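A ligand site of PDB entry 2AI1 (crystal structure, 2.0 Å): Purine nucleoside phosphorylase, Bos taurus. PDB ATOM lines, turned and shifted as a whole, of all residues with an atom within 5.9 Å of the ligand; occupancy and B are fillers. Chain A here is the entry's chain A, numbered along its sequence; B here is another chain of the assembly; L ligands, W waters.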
ATOM      1  N   CYS A  31      32.320   5.809  24.450  1.00  0.00           N
ATOM      2  CA  CYS A  31      33.195   6.875  23.982  1.00  0.00           C
ATOM      3  C   CYS A  31      33.131   7.115  22.474  1.00  0.00           C
ATOM      4  O   CYS A  31      33.351   6.212  21.673  1.00  0.00           O
ATOM      5  CB  CYS A  31      34.638   6.546  24.384  1.00  0.00           C
ATOM      6  SG  CYS A  31      34.888   6.289  26.176  1.00  0.00           S
ATOM      7  N   GLY A  32      32.805   8.360  22.112  1.00  0.00           N
ATOM      8  CA  GLY A  32      32.726   8.723  20.710  1.00  0.00           C
ATOM      9  C   GLY A  32      34.097   8.872  20.082  1.00  0.00           C
ATOM     10  O   GLY A  32      35.116   8.613  20.722  1.00  0.00           O
ATOM     11  N   SER A  33      34.137   9.317  18.822  1.00  0.00           N
ATOM     12  CA  SER A  33      35.414   9.481  18.122  1.00  0.00           C
ATOM     13  C   SER A  33      36.306  10.536  18.761  1.00  0.00           C
ATOM     14  O   SER A  33      35.892  11.675  18.995  1.00  0.00           O
ATOM     15  CB  SER A  33      35.158   9.839  16.652  1.00  0.00           C
ATOM     16  OG  SER A  33      34.414  11.036  16.555  1.00  0.00           O
ATOM     17  N   ARG A  84      32.749   2.779  19.161  1.00  0.00           N
ATOM     18  CA  ARG A  84      31.366   2.328  19.059  1.00  0.00           C
ATOM     19  C   ARG A  84      31.066   1.890  17.634  1.00  0.00           C
ATOM     20  O   ARG A  84      31.948   1.932  16.772  1.00  0.00           O
ATOM     21  CB  ARG A  84      30.399   3.441  19.462  1.00  0.00           C
ATOM     22  CG  ARG A  84      30.536   4.718  18.625  1.00  0.00           C
ATOM     23  CD  ARG A  84      29.167   5.296  18.269  1.00  0.00           C
ATOM     24  NE  ARG A  84      28.400   5.671  19.451  1.00  0.00           N
ATOM     25  CZ  ARG A  84      28.622   6.751  20.185  1.00  0.00           C
ATOM     26  NH1 ARG A  84      29.600   7.595  19.858  1.00  0.00           N
ATOM     27  NH2 ARG A  84      27.888   6.990  21.256  1.00  0.00           N
ATOM     28  N   HIS A  86      28.478   2.035  14.051  1.00  0.00           N
ATOM     29  CA  HIS A  86      27.661   2.994  13.300  1.00  0.00           C
ATOM     30  C   HIS A  86      26.828   2.385  12.183  1.00  0.00           C
ATOM     31  O   HIS A  86      27.207   1.399  11.556  1.00  0.00           O
ATOM     32  CB  HIS A  86      28.534   4.091  12.680  1.00  0.00           C
ATOM     33  CG  HIS A  86      29.432   4.797  13.661  1.00  0.00           C
ATOM     34  ND1 HIS A  86      30.715   4.377  13.923  1.00  0.00           N
ATOM     35  CD2 HIS A  86      29.211   5.884  14.438  1.00  0.00           C
ATOM     36  CE1 HIS A  86      31.258   5.184  14.829  1.00  0.00           C
ATOM     37  NE2 HIS A  86      30.369   6.099  15.151  1.00  0.00           N
ATOM     38  N   TYR A  88      26.364   3.717   9.320  1.00  0.00           N
ATOM     39  CA  TYR A  88      27.058   3.880   8.049  1.00  0.00           C
ATOM     40  C   TYR A  88      28.076   2.786   7.748  1.00  0.00           C
ATOM     41  O   TYR A  88      28.595   2.709   6.635  1.00  0.00           O
ATOM     42  CB  TYR A  88      27.699   5.282   7.949  1.00  0.00           C
ATOM     43  CG  TYR A  88      28.785   5.593   8.967  1.00  0.00           C
ATOM     44  CD1 TYR A  88      30.007   4.909   8.969  1.00  0.00           C
ATOM     45  CD2 TYR A  88      28.601   6.598   9.924  1.00  0.00           C
ATOM     46  CE1 TYR A  88      31.017   5.218   9.894  1.00  0.00           C
ATOM     47  CE2 TYR A  88      29.614   6.920  10.848  1.00  0.00           C
ATOM     48  CZ  TYR A  88      30.808   6.224  10.816  1.00  0.00           C
ATOM     49  OH  TYR A  88      31.798   6.549  11.722  1.00  0.00           O
ATOM     50  N   THR A 114      28.664   9.759  24.651  1.00  0.00           N
ATOM     51  CA  THR A 114      29.392  10.916  24.155  1.00  0.00           C
ATOM     52  C   THR A 114      29.607  10.774  22.658  1.00  0.00           C
ATOM     53  O   THR A 114      29.627   9.667  22.127  1.00  0.00           O
ATOM     54  CB  THR A 114      30.780  11.036  24.814  1.00  0.00           C
ATOM     55  OG1 THR A 114      31.636   9.999  24.315  1.00  0.00           O
ATOM     56  CG2 THR A 114      30.666  10.904  26.332  1.00  0.00           C
ATOM     57  N   ASN A 115      29.757  11.904  21.973  1.00  0.00           N
ATOM     58  CA  ASN A 115      29.980  11.868  20.532  1.00  0.00           C
ATOM     59  C   ASN A 115      30.612  13.149  20.026  1.00  0.00           C
ATOM     60  O   ASN A 115      30.669  14.154  20.734  1.00  0.00           O
ATOM     61  CB  ASN A 115      28.654  11.644  19.787  1.00  0.00           C
ATOM     62  CG  ASN A 115      27.679  12.804  19.958  1.00  0.00           C
ATOM     63  OD1 ASN A 115      28.006  13.947  19.656  1.00  0.00           O
ATOM     64  ND2 ASN A 115      26.474  12.501  20.437  1.00  0.00           N
ATOM     65  N   ALA A 116      31.091  13.090  18.787  1.00  0.00           N
ATOM     66  CA  ALA A 116      31.679  14.249  18.122  1.00  0.00           C
ATOM     67  C   ALA A 116      30.582  14.715  17.179  1.00  0.00           C
ATOM     68  O   ALA A 116      29.972  13.901  16.481  1.00  0.00           O
ATOM     69  CB  ALA A 116      32.907  13.824  17.327  1.00  0.00           C
ATOM     70  N   ALA A 117      30.312  16.014  17.147  1.00  0.00           N
ATOM     71  CA  ALA A 117      29.245  16.525  16.296  1.00  0.00           C
ATOM     72  C   ALA A 117      29.560  17.857  15.630  1.00  0.00           C
ATOM     73  O   ALA A 117      30.500  18.556  16.018  1.00  0.00           O
ATOM     74  CB  ALA A 117      27.956  16.661  17.128  1.00  0.00           C
ATOM     75  N   GLY A 118      28.774  18.184  14.611  1.00  0.00           N
ATOM     76  CA  GLY A 118      28.937  19.440  13.901  1.00  0.00           C
ATOM     77  C   GLY A 118      27.955  20.445  14.501  1.00  0.00           C
ATOM     78  O   GLY A 118      26.791  20.103  14.764  1.00  0.00           O
ATOM     79  N   GLY A 119      28.412  21.676  14.711  1.00  0.00           N
ATOM     80  CA  GLY A 119      27.546  22.683  15.309  1.00  0.00           C
ATOM     81  C   GLY A 119      26.602  23.394  14.360  1.00  0.00           C
ATOM     82  O   GLY A 119      27.029  23.947  13.335  1.00  0.00           O
ATOM     83  N   TYR A 192      20.203  17.286  19.745  1.00  0.00           N
ATOM     84  CA  TYR A 192      21.091  16.551  18.836  1.00  0.00           C
ATOM     85  C   TYR A 192      20.273  15.801  17.792  1.00  0.00           C
ATOM     86  O   TYR A 192      19.342  15.073  18.132  1.00  0.00           O
ATOM     87  CB  TYR A 192      21.941  15.555  19.640  1.00  0.00           C
ATOM     88  CG  TYR A 192      22.788  14.580  18.824  1.00  0.00           C
ATOM     89  CD1 TYR A 192      22.255  13.391  18.325  1.00  0.00           C
ATOM     90  CD2 TYR A 192      24.138  14.847  18.580  1.00  0.00           C
ATOM     91  CE1 TYR A 192      23.058  12.472  17.617  1.00  0.00           C
ATOM     92  CE2 TYR A 192      24.943  13.948  17.861  1.00  0.00           C
ATOM     93  CZ  TYR A 192      24.404  12.759  17.392  1.00  0.00           C
ATOM     94  OH  TYR A 192      25.216  11.873  16.712  1.00  0.00           O
ATOM     95  N   LEU A 195      21.638  11.582  11.727  1.00  0.00           N
ATOM     96  CA  LEU A 195      21.358  11.163  10.358  1.00  0.00           C
ATOM     97  C   LEU A 195      22.372  10.050  10.025  1.00  0.00           C
ATOM     98  O   LEU A 195      23.391   9.890  10.716  1.00  0.00           O
ATOM     99  CB  LEU A 195      21.453  12.336   9.377  1.00  0.00           C
ATOM    100  CG  LEU A 195      22.574  13.369   9.442  1.00  0.00           C
ATOM    101  CD1 LEU A 195      23.910  12.696   9.169  1.00  0.00           C
ATOM    102  CD2 LEU A 195      22.293  14.458   8.415  1.00  0.00           C
ATOM    103  N   ASN A 199      28.687  10.716   4.520  1.00  0.00           N
ATOM    104  CA  ASN A 199      29.096  12.013   3.977  1.00  0.00           C
ATOM    105  C   ASN A 199      28.655  13.164   4.861  1.00  0.00           C
ATOM    106  O   ASN A 199      27.716  13.037   5.658  1.00  0.00           O
ATOM    107  CB  ASN A 199      28.509  12.244   2.575  1.00  0.00           C
ATOM    108  CG  ASN A 199      26.984  12.297   2.566  1.00  0.00           C
ATOM    109  OD1 ASN A 199      26.331  11.252   2.517  1.00  0.00           O
ATOM    110  ND2 ASN A 199      26.416  13.494   2.633  1.00  0.00           N
ATOM    111  N   PHE A 200      29.340  14.306   4.727  1.00  0.00           N
ATOM    112  CA  PHE A 200      28.985  15.498   5.486  1.00  0.00           C
ATOM    113  C   PHE A 200      27.856  16.205   4.739  1.00  0.00           C
ATOM    114  O   PHE A 200      27.738  16.088   3.511  1.00  0.00           O
ATOM    115  CB  PHE A 200      30.180  16.447   5.619  1.00  0.00           C
ATOM    116  CG  PHE A 200      31.223  15.972   6.582  1.00  0.00           C
ATOM    117  CD1 PHE A 200      32.433  15.481   6.123  1.00  0.00           C
ATOM    118  CD2 PHE A 200      30.986  16.021   7.955  1.00  0.00           C
ATOM    119  CE1 PHE A 200      33.417  15.057   7.024  1.00  0.00           C
ATOM    120  CE2 PHE A 200      31.956  15.594   8.856  1.00  0.00           C
ATOM    121  CZ  PHE A 200      33.172  15.107   8.385  1.00  0.00           C
ATOM    122  N   GLU A 201      27.051  16.951   5.481  1.00  0.00           N
ATOM    123  CA  GLU A 201      25.896  17.661   4.939  1.00  0.00           C
ATOM    124  C   GLU A 201      26.195  18.801   3.957  1.00  0.00           C
ATOM    125  O   GLU A 201      27.242  19.439   4.033  1.00  0.00           O
ATOM    126  CB  GLU A 201      25.046  18.227   6.085  1.00  0.00           C
ATOM    127  CG  GLU A 201      24.507  17.179   7.052  1.00  0.00           C
ATOM    128  CD  GLU A 201      25.570  16.640   7.991  1.00  0.00           C
ATOM    129  OE1 GLU A 201      25.476  15.445   8.347  1.00  0.00           O
ATOM    130  OE2 GLU A 201      26.491  17.393   8.393  1.00  0.00           O
ATOM    131  N   VAL A 217      24.617  18.180  14.906  1.00  0.00           N
ATOM    132  CA  VAL A 217      24.352  17.058  14.005  1.00  0.00           C
ATOM    133  C   VAL A 217      25.433  15.965  14.079  1.00  0.00           C
ATOM    134  O   VAL A 217      26.634  16.268  14.064  1.00  0.00           O
ATOM    135  CB  VAL A 217      24.216  17.552  12.531  1.00  0.00           C
ATOM    136  CG1 VAL A 217      25.461  18.321  12.116  1.00  0.00           C
ATOM    137  CG2 VAL A 217      23.958  16.360  11.590  1.00  0.00           C
ATOM    138  N   GLY A 218      25.008  14.701  14.181  1.00  0.00           N
ATOM    139  CA  GLY A 218      25.944  13.579  14.267  1.00  0.00           C
ATOM    140  C   GLY A 218      25.446  12.298  13.615  1.00  0.00           C
ATOM    141  O   GLY A 218      24.365  12.277  13.023  1.00  0.00           O
ATOM    142  N   MET A 219      26.227  11.227  13.723  1.00  0.00           N
ATOM    143  CA  MET A 219      25.868   9.947  13.104  1.00  0.00           C
ATOM    144  C   MET A 219      25.712   8.749  14.050  1.00  0.00           C
ATOM    145  O   MET A 219      25.805   7.601  13.614  1.00  0.00           O
ATOM    146  CB  MET A 219      26.921   9.589  12.029  1.00  0.00           C
ATOM    147  CG  MET A 219      27.122  10.661  10.966  1.00  0.00           C
ATOM    148  SD  MET A 219      28.493  10.260   9.820  1.00  0.00           S
ATOM    149  CE  MET A 219      28.690  11.797   8.945  1.00  0.00           C
ATOM    150  N   SER A 220      25.464   9.010  15.330  1.00  0.00           N
ATOM    151  CA  SER A 220      25.335   7.921  16.302  1.00  0.00           C
ATOM    152  C   SER A 220      24.452   8.294  17.484  1.00  0.00           C
ATOM    153  O   SER A 220      23.576   9.155  17.388  1.00  0.00           O
ATOM    154  CB  SER A 220      26.722   7.586  16.852  1.00  0.00           C
ATOM    155  OG  SER A 220      27.169   8.660  17.674  1.00  0.00           O
ATOM    156  N   THR A 221      24.680   7.608  18.611  1.00  0.00           N
ATOM    157  CA  THR A 221      23.989   7.922  19.868  1.00  0.00           C
ATOM    158  C   THR A 221      22.498   7.657  20.055  1.00  0.00           C
ATOM    159  O   THR A 221      22.100   6.921  20.956  1.00  0.00           O
ATOM    160  CB  THR A 221      24.245   9.391  20.217  1.00  0.00           C
ATOM    161  OG1 THR A 221      25.655   9.613  20.221  1.00  0.00           O
ATOM    162  CG2 THR A 221      23.660   9.748  21.582  1.00  0.00           C
ATOM    163  N   THR A 242      32.965  19.628  17.180  1.00  0.00           N
ATOM    164  CA  THR A 242      34.238  19.555  16.454  1.00  0.00           C
ATOM    165  C   THR A 242      34.378  20.485  15.260  1.00  0.00           C
ATOM    166  O   THR A 242      35.478  20.636  14.723  1.00  0.00           O
ATOM    167  CB  THR A 242      34.532  18.103  15.998  1.00  0.00           C
ATOM    168  OG1 THR A 242      33.430  17.603  15.227  1.00  0.00           O
ATOM    169  CG2 THR A 242      34.747  17.213  17.216  1.00  0.00           C
ATOM    170  N   ASN A 243      33.280  21.104  14.841  1.00  0.00           N
ATOM    171  CA  ASN A 243      33.317  22.025  13.709  1.00  0.00           C
ATOM    172  C   ASN A 243      31.994  22.757  13.529  1.00  0.00           C
ATOM    173  O   ASN A 243      30.935  22.234  13.872  1.00  0.00           O
ATOM    174  CB  ASN A 243      33.662  21.280  12.407  1.00  0.00           C
ATOM    175  CG  ASN A 243      32.574  20.302  11.979  1.00  0.00           C
ATOM    176  OD1 ASN A 243      32.395  19.249  12.591  1.00  0.00           O
ATOM    177  ND2 ASN A 243      31.848  20.648  10.921  1.00  0.00           N
ATOM    178  N   VAL A 245      29.379  23.802  11.068  1.00  0.00           N
ATOM    179  CA  VAL A 245      28.929  23.431   9.720  1.00  0.00           C
ATOM    180  C   VAL A 245      28.740  24.649   8.804  1.00  0.00           C
ATOM    181  O   VAL A 245      28.305  25.706   9.248  1.00  0.00           O
ATOM    182  CB  VAL A 245      27.604  22.638   9.770  1.00  0.00           C
ATOM    183  CG1 VAL A 245      27.723  21.484  10.751  1.00  0.00           C
ATOM    184  CG2 VAL A 245      26.450  23.553  10.136  1.00  0.00           C
ATOM    185  N   ALA A 255      33.872  20.876   5.660  1.00  0.00           N
ATOM    186  CA  ALA A 255      34.064  19.847   6.669  1.00  0.00           C
ATOM    187  C   ALA A 255      35.043  18.745   6.258  1.00  0.00           C
ATOM    188  O   ALA A 255      35.050  18.296   5.103  1.00  0.00           O
ATOM    189  CB  ALA A 255      32.724  19.226   7.040  1.00  0.00           C
ATOM    190  N   ASN A 256      35.864  18.312   7.209  1.00  0.00           N
ATOM    191  CA  ASN A 256      36.846  17.265   6.975  1.00  0.00           C
ATOM    192  C   ASN A 256      37.112  16.521   8.289  1.00  0.00           C
ATOM    193  O   ASN A 256      37.163  17.130   9.354  1.00  0.00           O
ATOM    194  CB  ASN A 256      38.153  17.864   6.439  1.00  0.00           C
ATOM    195  CG  ASN A 256      38.838  18.765   7.438  1.00  0.00           C
ATOM    196  OD1 ASN A 256      39.321  18.308   8.472  1.00  0.00           O
ATOM    197  ND2 ASN A 256      38.869  20.060   7.151  1.00  0.00           N
ATOM    198  N   HIS A 257      37.276  15.207   8.196  1.00  0.00           N
ATOM    199  CA  HIS A 257      37.503  14.380   9.372  1.00  0.00           C
ATOM    200  C   HIS A 257      38.792  14.701  10.135  1.00  0.00           C
ATOM    201  O   HIS A 257      38.895  14.443  11.335  1.00  0.00           O
ATOM    202  CB  HIS A 257      37.502  12.900   8.971  1.00  0.00           C
ATOM    203  CG  HIS A 257      37.500  11.959  10.131  1.00  0.00           C
ATOM    204  ND1 HIS A 257      36.547  12.000  11.118  1.00  0.00           N
ATOM    205  CD2 HIS A 257      38.337  10.943  10.457  1.00  0.00           C
ATOM    206  CE1 HIS A 257      36.794  11.052  12.007  1.00  0.00           C
ATOM    207  NE2 HIS A 257      37.872  10.399  11.627  1.00  0.00           N
ATOM    208  N   VAL A 260      38.189  17.270  12.710  1.00  0.00           N
ATOM    209  CA  VAL A 260      37.309  16.694  13.725  1.00  0.00           C
ATOM    210  C   VAL A 260      38.149  15.947  14.753  1.00  0.00           C
ATOM    211  O   VAL A 260      37.890  16.024  15.962  1.00  0.00           O
ATOM    212  CB  VAL A 260      36.280  15.727  13.095  1.00  0.00           C
ATOM    213  CG1 VAL A 260      35.426  15.090  14.186  1.00  0.00           C
ATOM    214  CG2 VAL A 260      35.399  16.470  12.104  1.00  0.00           C
ATOM    215  N   PHE B 159      34.685   9.716   5.015  1.00  0.00           N
ATOM    216  CA  PHE B 159      33.731  10.822   5.213  1.00  0.00           C
ATOM    217  C   PHE B 159      33.888  11.938   4.190  1.00  0.00           C
ATOM    218  O   PHE B 159      34.458  12.988   4.492  1.00  0.00           O
ATOM    219  CB  PHE B 159      33.891  11.445   6.598  1.00  0.00           C
ATOM    220  CG  PHE B 159      33.826  10.458   7.732  1.00  0.00           C
ATOM    221  CD1 PHE B 159      34.980  10.101   8.424  1.00  0.00           C
ATOM    222  CD2 PHE B 159      32.616   9.906   8.117  1.00  0.00           C
ATOM    223  CE1 PHE B 159      34.942   9.198   9.489  1.00  0.00           C
ATOM    224  CE2 PHE B 159      32.550   9.003   9.176  1.00  0.00           C
ATOM    225  CZ  PHE B 159      33.717   8.649   9.868  1.00  0.00           C
HETATM  226  O1  LIG L   1      31.548  10.298  17.948  1.00  0.00           O
HETATM  227  P1  LIG L   1      30.706   9.539  16.818  1.00  0.00           P
HETATM  228  O2  LIG L   1      30.788   7.963  17.145  1.00  0.00           O
HETATM  229  O3  LIG L   1      29.303   9.988  16.757  1.00  0.00           O
HETATM  230  C1  LIG L   1      31.555   9.815  15.248  1.00  0.00           C
HETATM  231  C2  LIG L   1      30.607   9.645  14.043  1.00  0.00           C
HETATM  232  O4  LIG L   1      31.331   9.623  12.801  1.00  0.00           O
HETATM  233  O5  LIG L   1      29.646  10.694  13.853  1.00  0.00           O
HETATM  234  C3  LIG L   1      30.171  11.656  12.920  1.00  0.00           C
HETATM  235  C4  LIG L   1      31.283  10.931  12.183  1.00  0.00           C
HETATM  236  C5  LIG L   1      32.557  11.729  12.433  1.00  0.00           C
HETATM  237  C6  LIG L   1      33.047  12.559  11.231  1.00  0.00           C
HETATM  238  O6  LIG L   1      34.239  13.294  11.569  1.00  0.00           O
HETATM  239  O7  LIG L   1      32.268  12.514  13.603  1.00  0.00           O
HETATM  240  C7  LIG L   1      30.858  12.846  13.588  1.00  0.00           C
HETATM  241  N1  LIG L   1      30.711  14.214  13.013  1.00  0.00           N
HETATM  242  C8  LIG L   1      31.570  15.198  13.271  1.00  0.00           C
HETATM  243  N2  LIG L   1      31.247  16.299  12.590  1.00  0.00           N
HETATM  244  C9  LIG L   1      30.157  16.013  11.889  1.00  0.00           C
HETATM  245  C10 LIG L   1      29.793  14.684  12.179  1.00  0.00           C
HETATM  246  N3  LIG L   1      28.639  14.130  11.707  1.00  0.00           N
HETATM  247  C11 LIG L   1      27.753  14.789  10.932  1.00  0.00           C
HETATM  248  N4  LIG L   1      26.577  14.292  10.560  1.00  0.00           N
HETATM  249  N5  LIG L   1      28.093  16.119  10.606  1.00  0.00           N
HETATM  250  C12 LIG L   1      29.278  16.722  11.075  1.00  0.00           C
HETATM  251  O8  LIG L   1      29.495  17.889  10.729  1.00  0.00           O
HETATM  252  O   HOH W   1      33.325   7.040  16.757  1.00  0.00           O
HETATM  253  O   HOH W   2      28.604  19.104   8.068  1.00  0.00           O
HETATM  254  O   HOH W   3      27.868  12.104  16.175  1.00  0.00           O
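Water W3 lies within hydrogen-bond range of O3 of the ligand (2.6 Å), OH of Tyr 192 (2.7 Å), O of Ala 116 (2.8 Å) and N of Met 219 (3.1 Å).
Water W1 lies within hydrogen-bond range of O2 of the ligand (2.7 Å), N of Ser 33 (3.2 Å) and NE2 of His 86 (3.5 Å).
Water W2 bridges the side-chain carboxylate (OE2) of Glu 201 (2.7 Å) and an oxygen (O8) of the ligand (3.1 Å).
The side-chain amide nitrogen (ND2) of Asn 115 is in hydrogen-bond range of the side-chain hydroxyl (OG1) of Thr 221, 3.0 Å away.
OG of Ser 220 is in hydrogen-bond range of NH1 of Arg 84 (3.4 Å).
OH of Tyr 88 lies within hydrogen-bond range of ND1 of His 86, 3.3 Å away.
N of Val 217 lies within hydrogen-bond range of O of Gly 118 (2.9 Å).
The side-chain hydroxyl (OG) of Ser 220 sits at hydrogen-bond distance from the side-chain hydroxyl (OG1) of Thr 221.
The side-chain hydroxyl (OH) of Tyr 192 is in hydrogen-bond range of the backbone NH (N) of Met 219.
O of Ala 117 is in hydrogen-bond range of N of Thr 242, at 2.9 Å.
The backbone NH (N) of Leu 195 is in hydrogen-bond range of the backbone carbonyl oxygen (O) of Gly 218 (3.1 Å).
Gly 32 touches the ligand (CA to O1, 3.4 Å).
CA of Asn 115 touches O1 of the ligand (3.4 Å).
Ala 117 touches the ligand (C to N2, 3.8 Å).
CA of Gly 118 touches O8 of the ligand (3.6 Å).
CD1 of Leu 195 touches N4 of the ligand (3.4 Å).
Phe 200 touches the ligand.
CG2 of Val 217 touches N4 of the ligand, 3.5 Å away.
CA of Gly 218 touches N3 of the ligand (3.8 Å).
Thr 242 touches the ligand (OG1 to C8, 3.6 Å).
Val 260 touches the ligand (CG1 to O6, 3.4 Å).
Phe 159 of chain B touches the ligand (CE2 to C4, 3.8 Å).
Hydrophobic or aromatic side chains within 4 Å of the ligand: His 86, Tyr 88, Ala 116, Leu 195, Phe 200, Val 217, Met 219, His 257, Val 260 and Phe 159 of chain B.
The nearest printed residue that does not touch the ligand is Val 245 (4.01 Å).
The guanidinium group (NH1) of Arg 84 lies within salt-bridge range of an oxygen (O2) of the ligand, at 3.0 Å.
An oxygen (O1) of the ligand lies within hydrogen-bond range of the backbone NH (N) of Ala 116.
A ring nitrogen (ND1) of His 257 sits at hydrogen-bond distance from an oxygen (O6) of the ligand, 2.7 Å away.
An oxygen (O1) of the ligand is in hydrogen-bond range of the side-chain hydroxyl (OG) of Ser 33 (3.3 Å).
O2 of the ligand sits at hydrogen-bond distance from NE2 of His 86 (2.8 Å).
The side-chain hydroxyl (OH) of Tyr 88 is in hydrogen-bond range of an oxygen (O4) of the ligand (3.3 Å).
The backbone NH (N) of Ser 33 is in hydrogen-bond range of an oxygen (O1) of the ligand (2.9 Å).
The side-chain hydroxyl (OG) of Ser 220 is in hydrogen-bond range of an oxygen (O3) of the ligand.
An oxygen (O5) of the ligand sits close to the backbone NH of Met 219, 3.5 Å away.
OD1 of Asn 243 sits close to N2 of the ligand (3.2 Å).
A nitrogen (N4) of the ligand lies within hydrogen-bond range of the side-chain carboxylate (OE1) of Glu 201.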
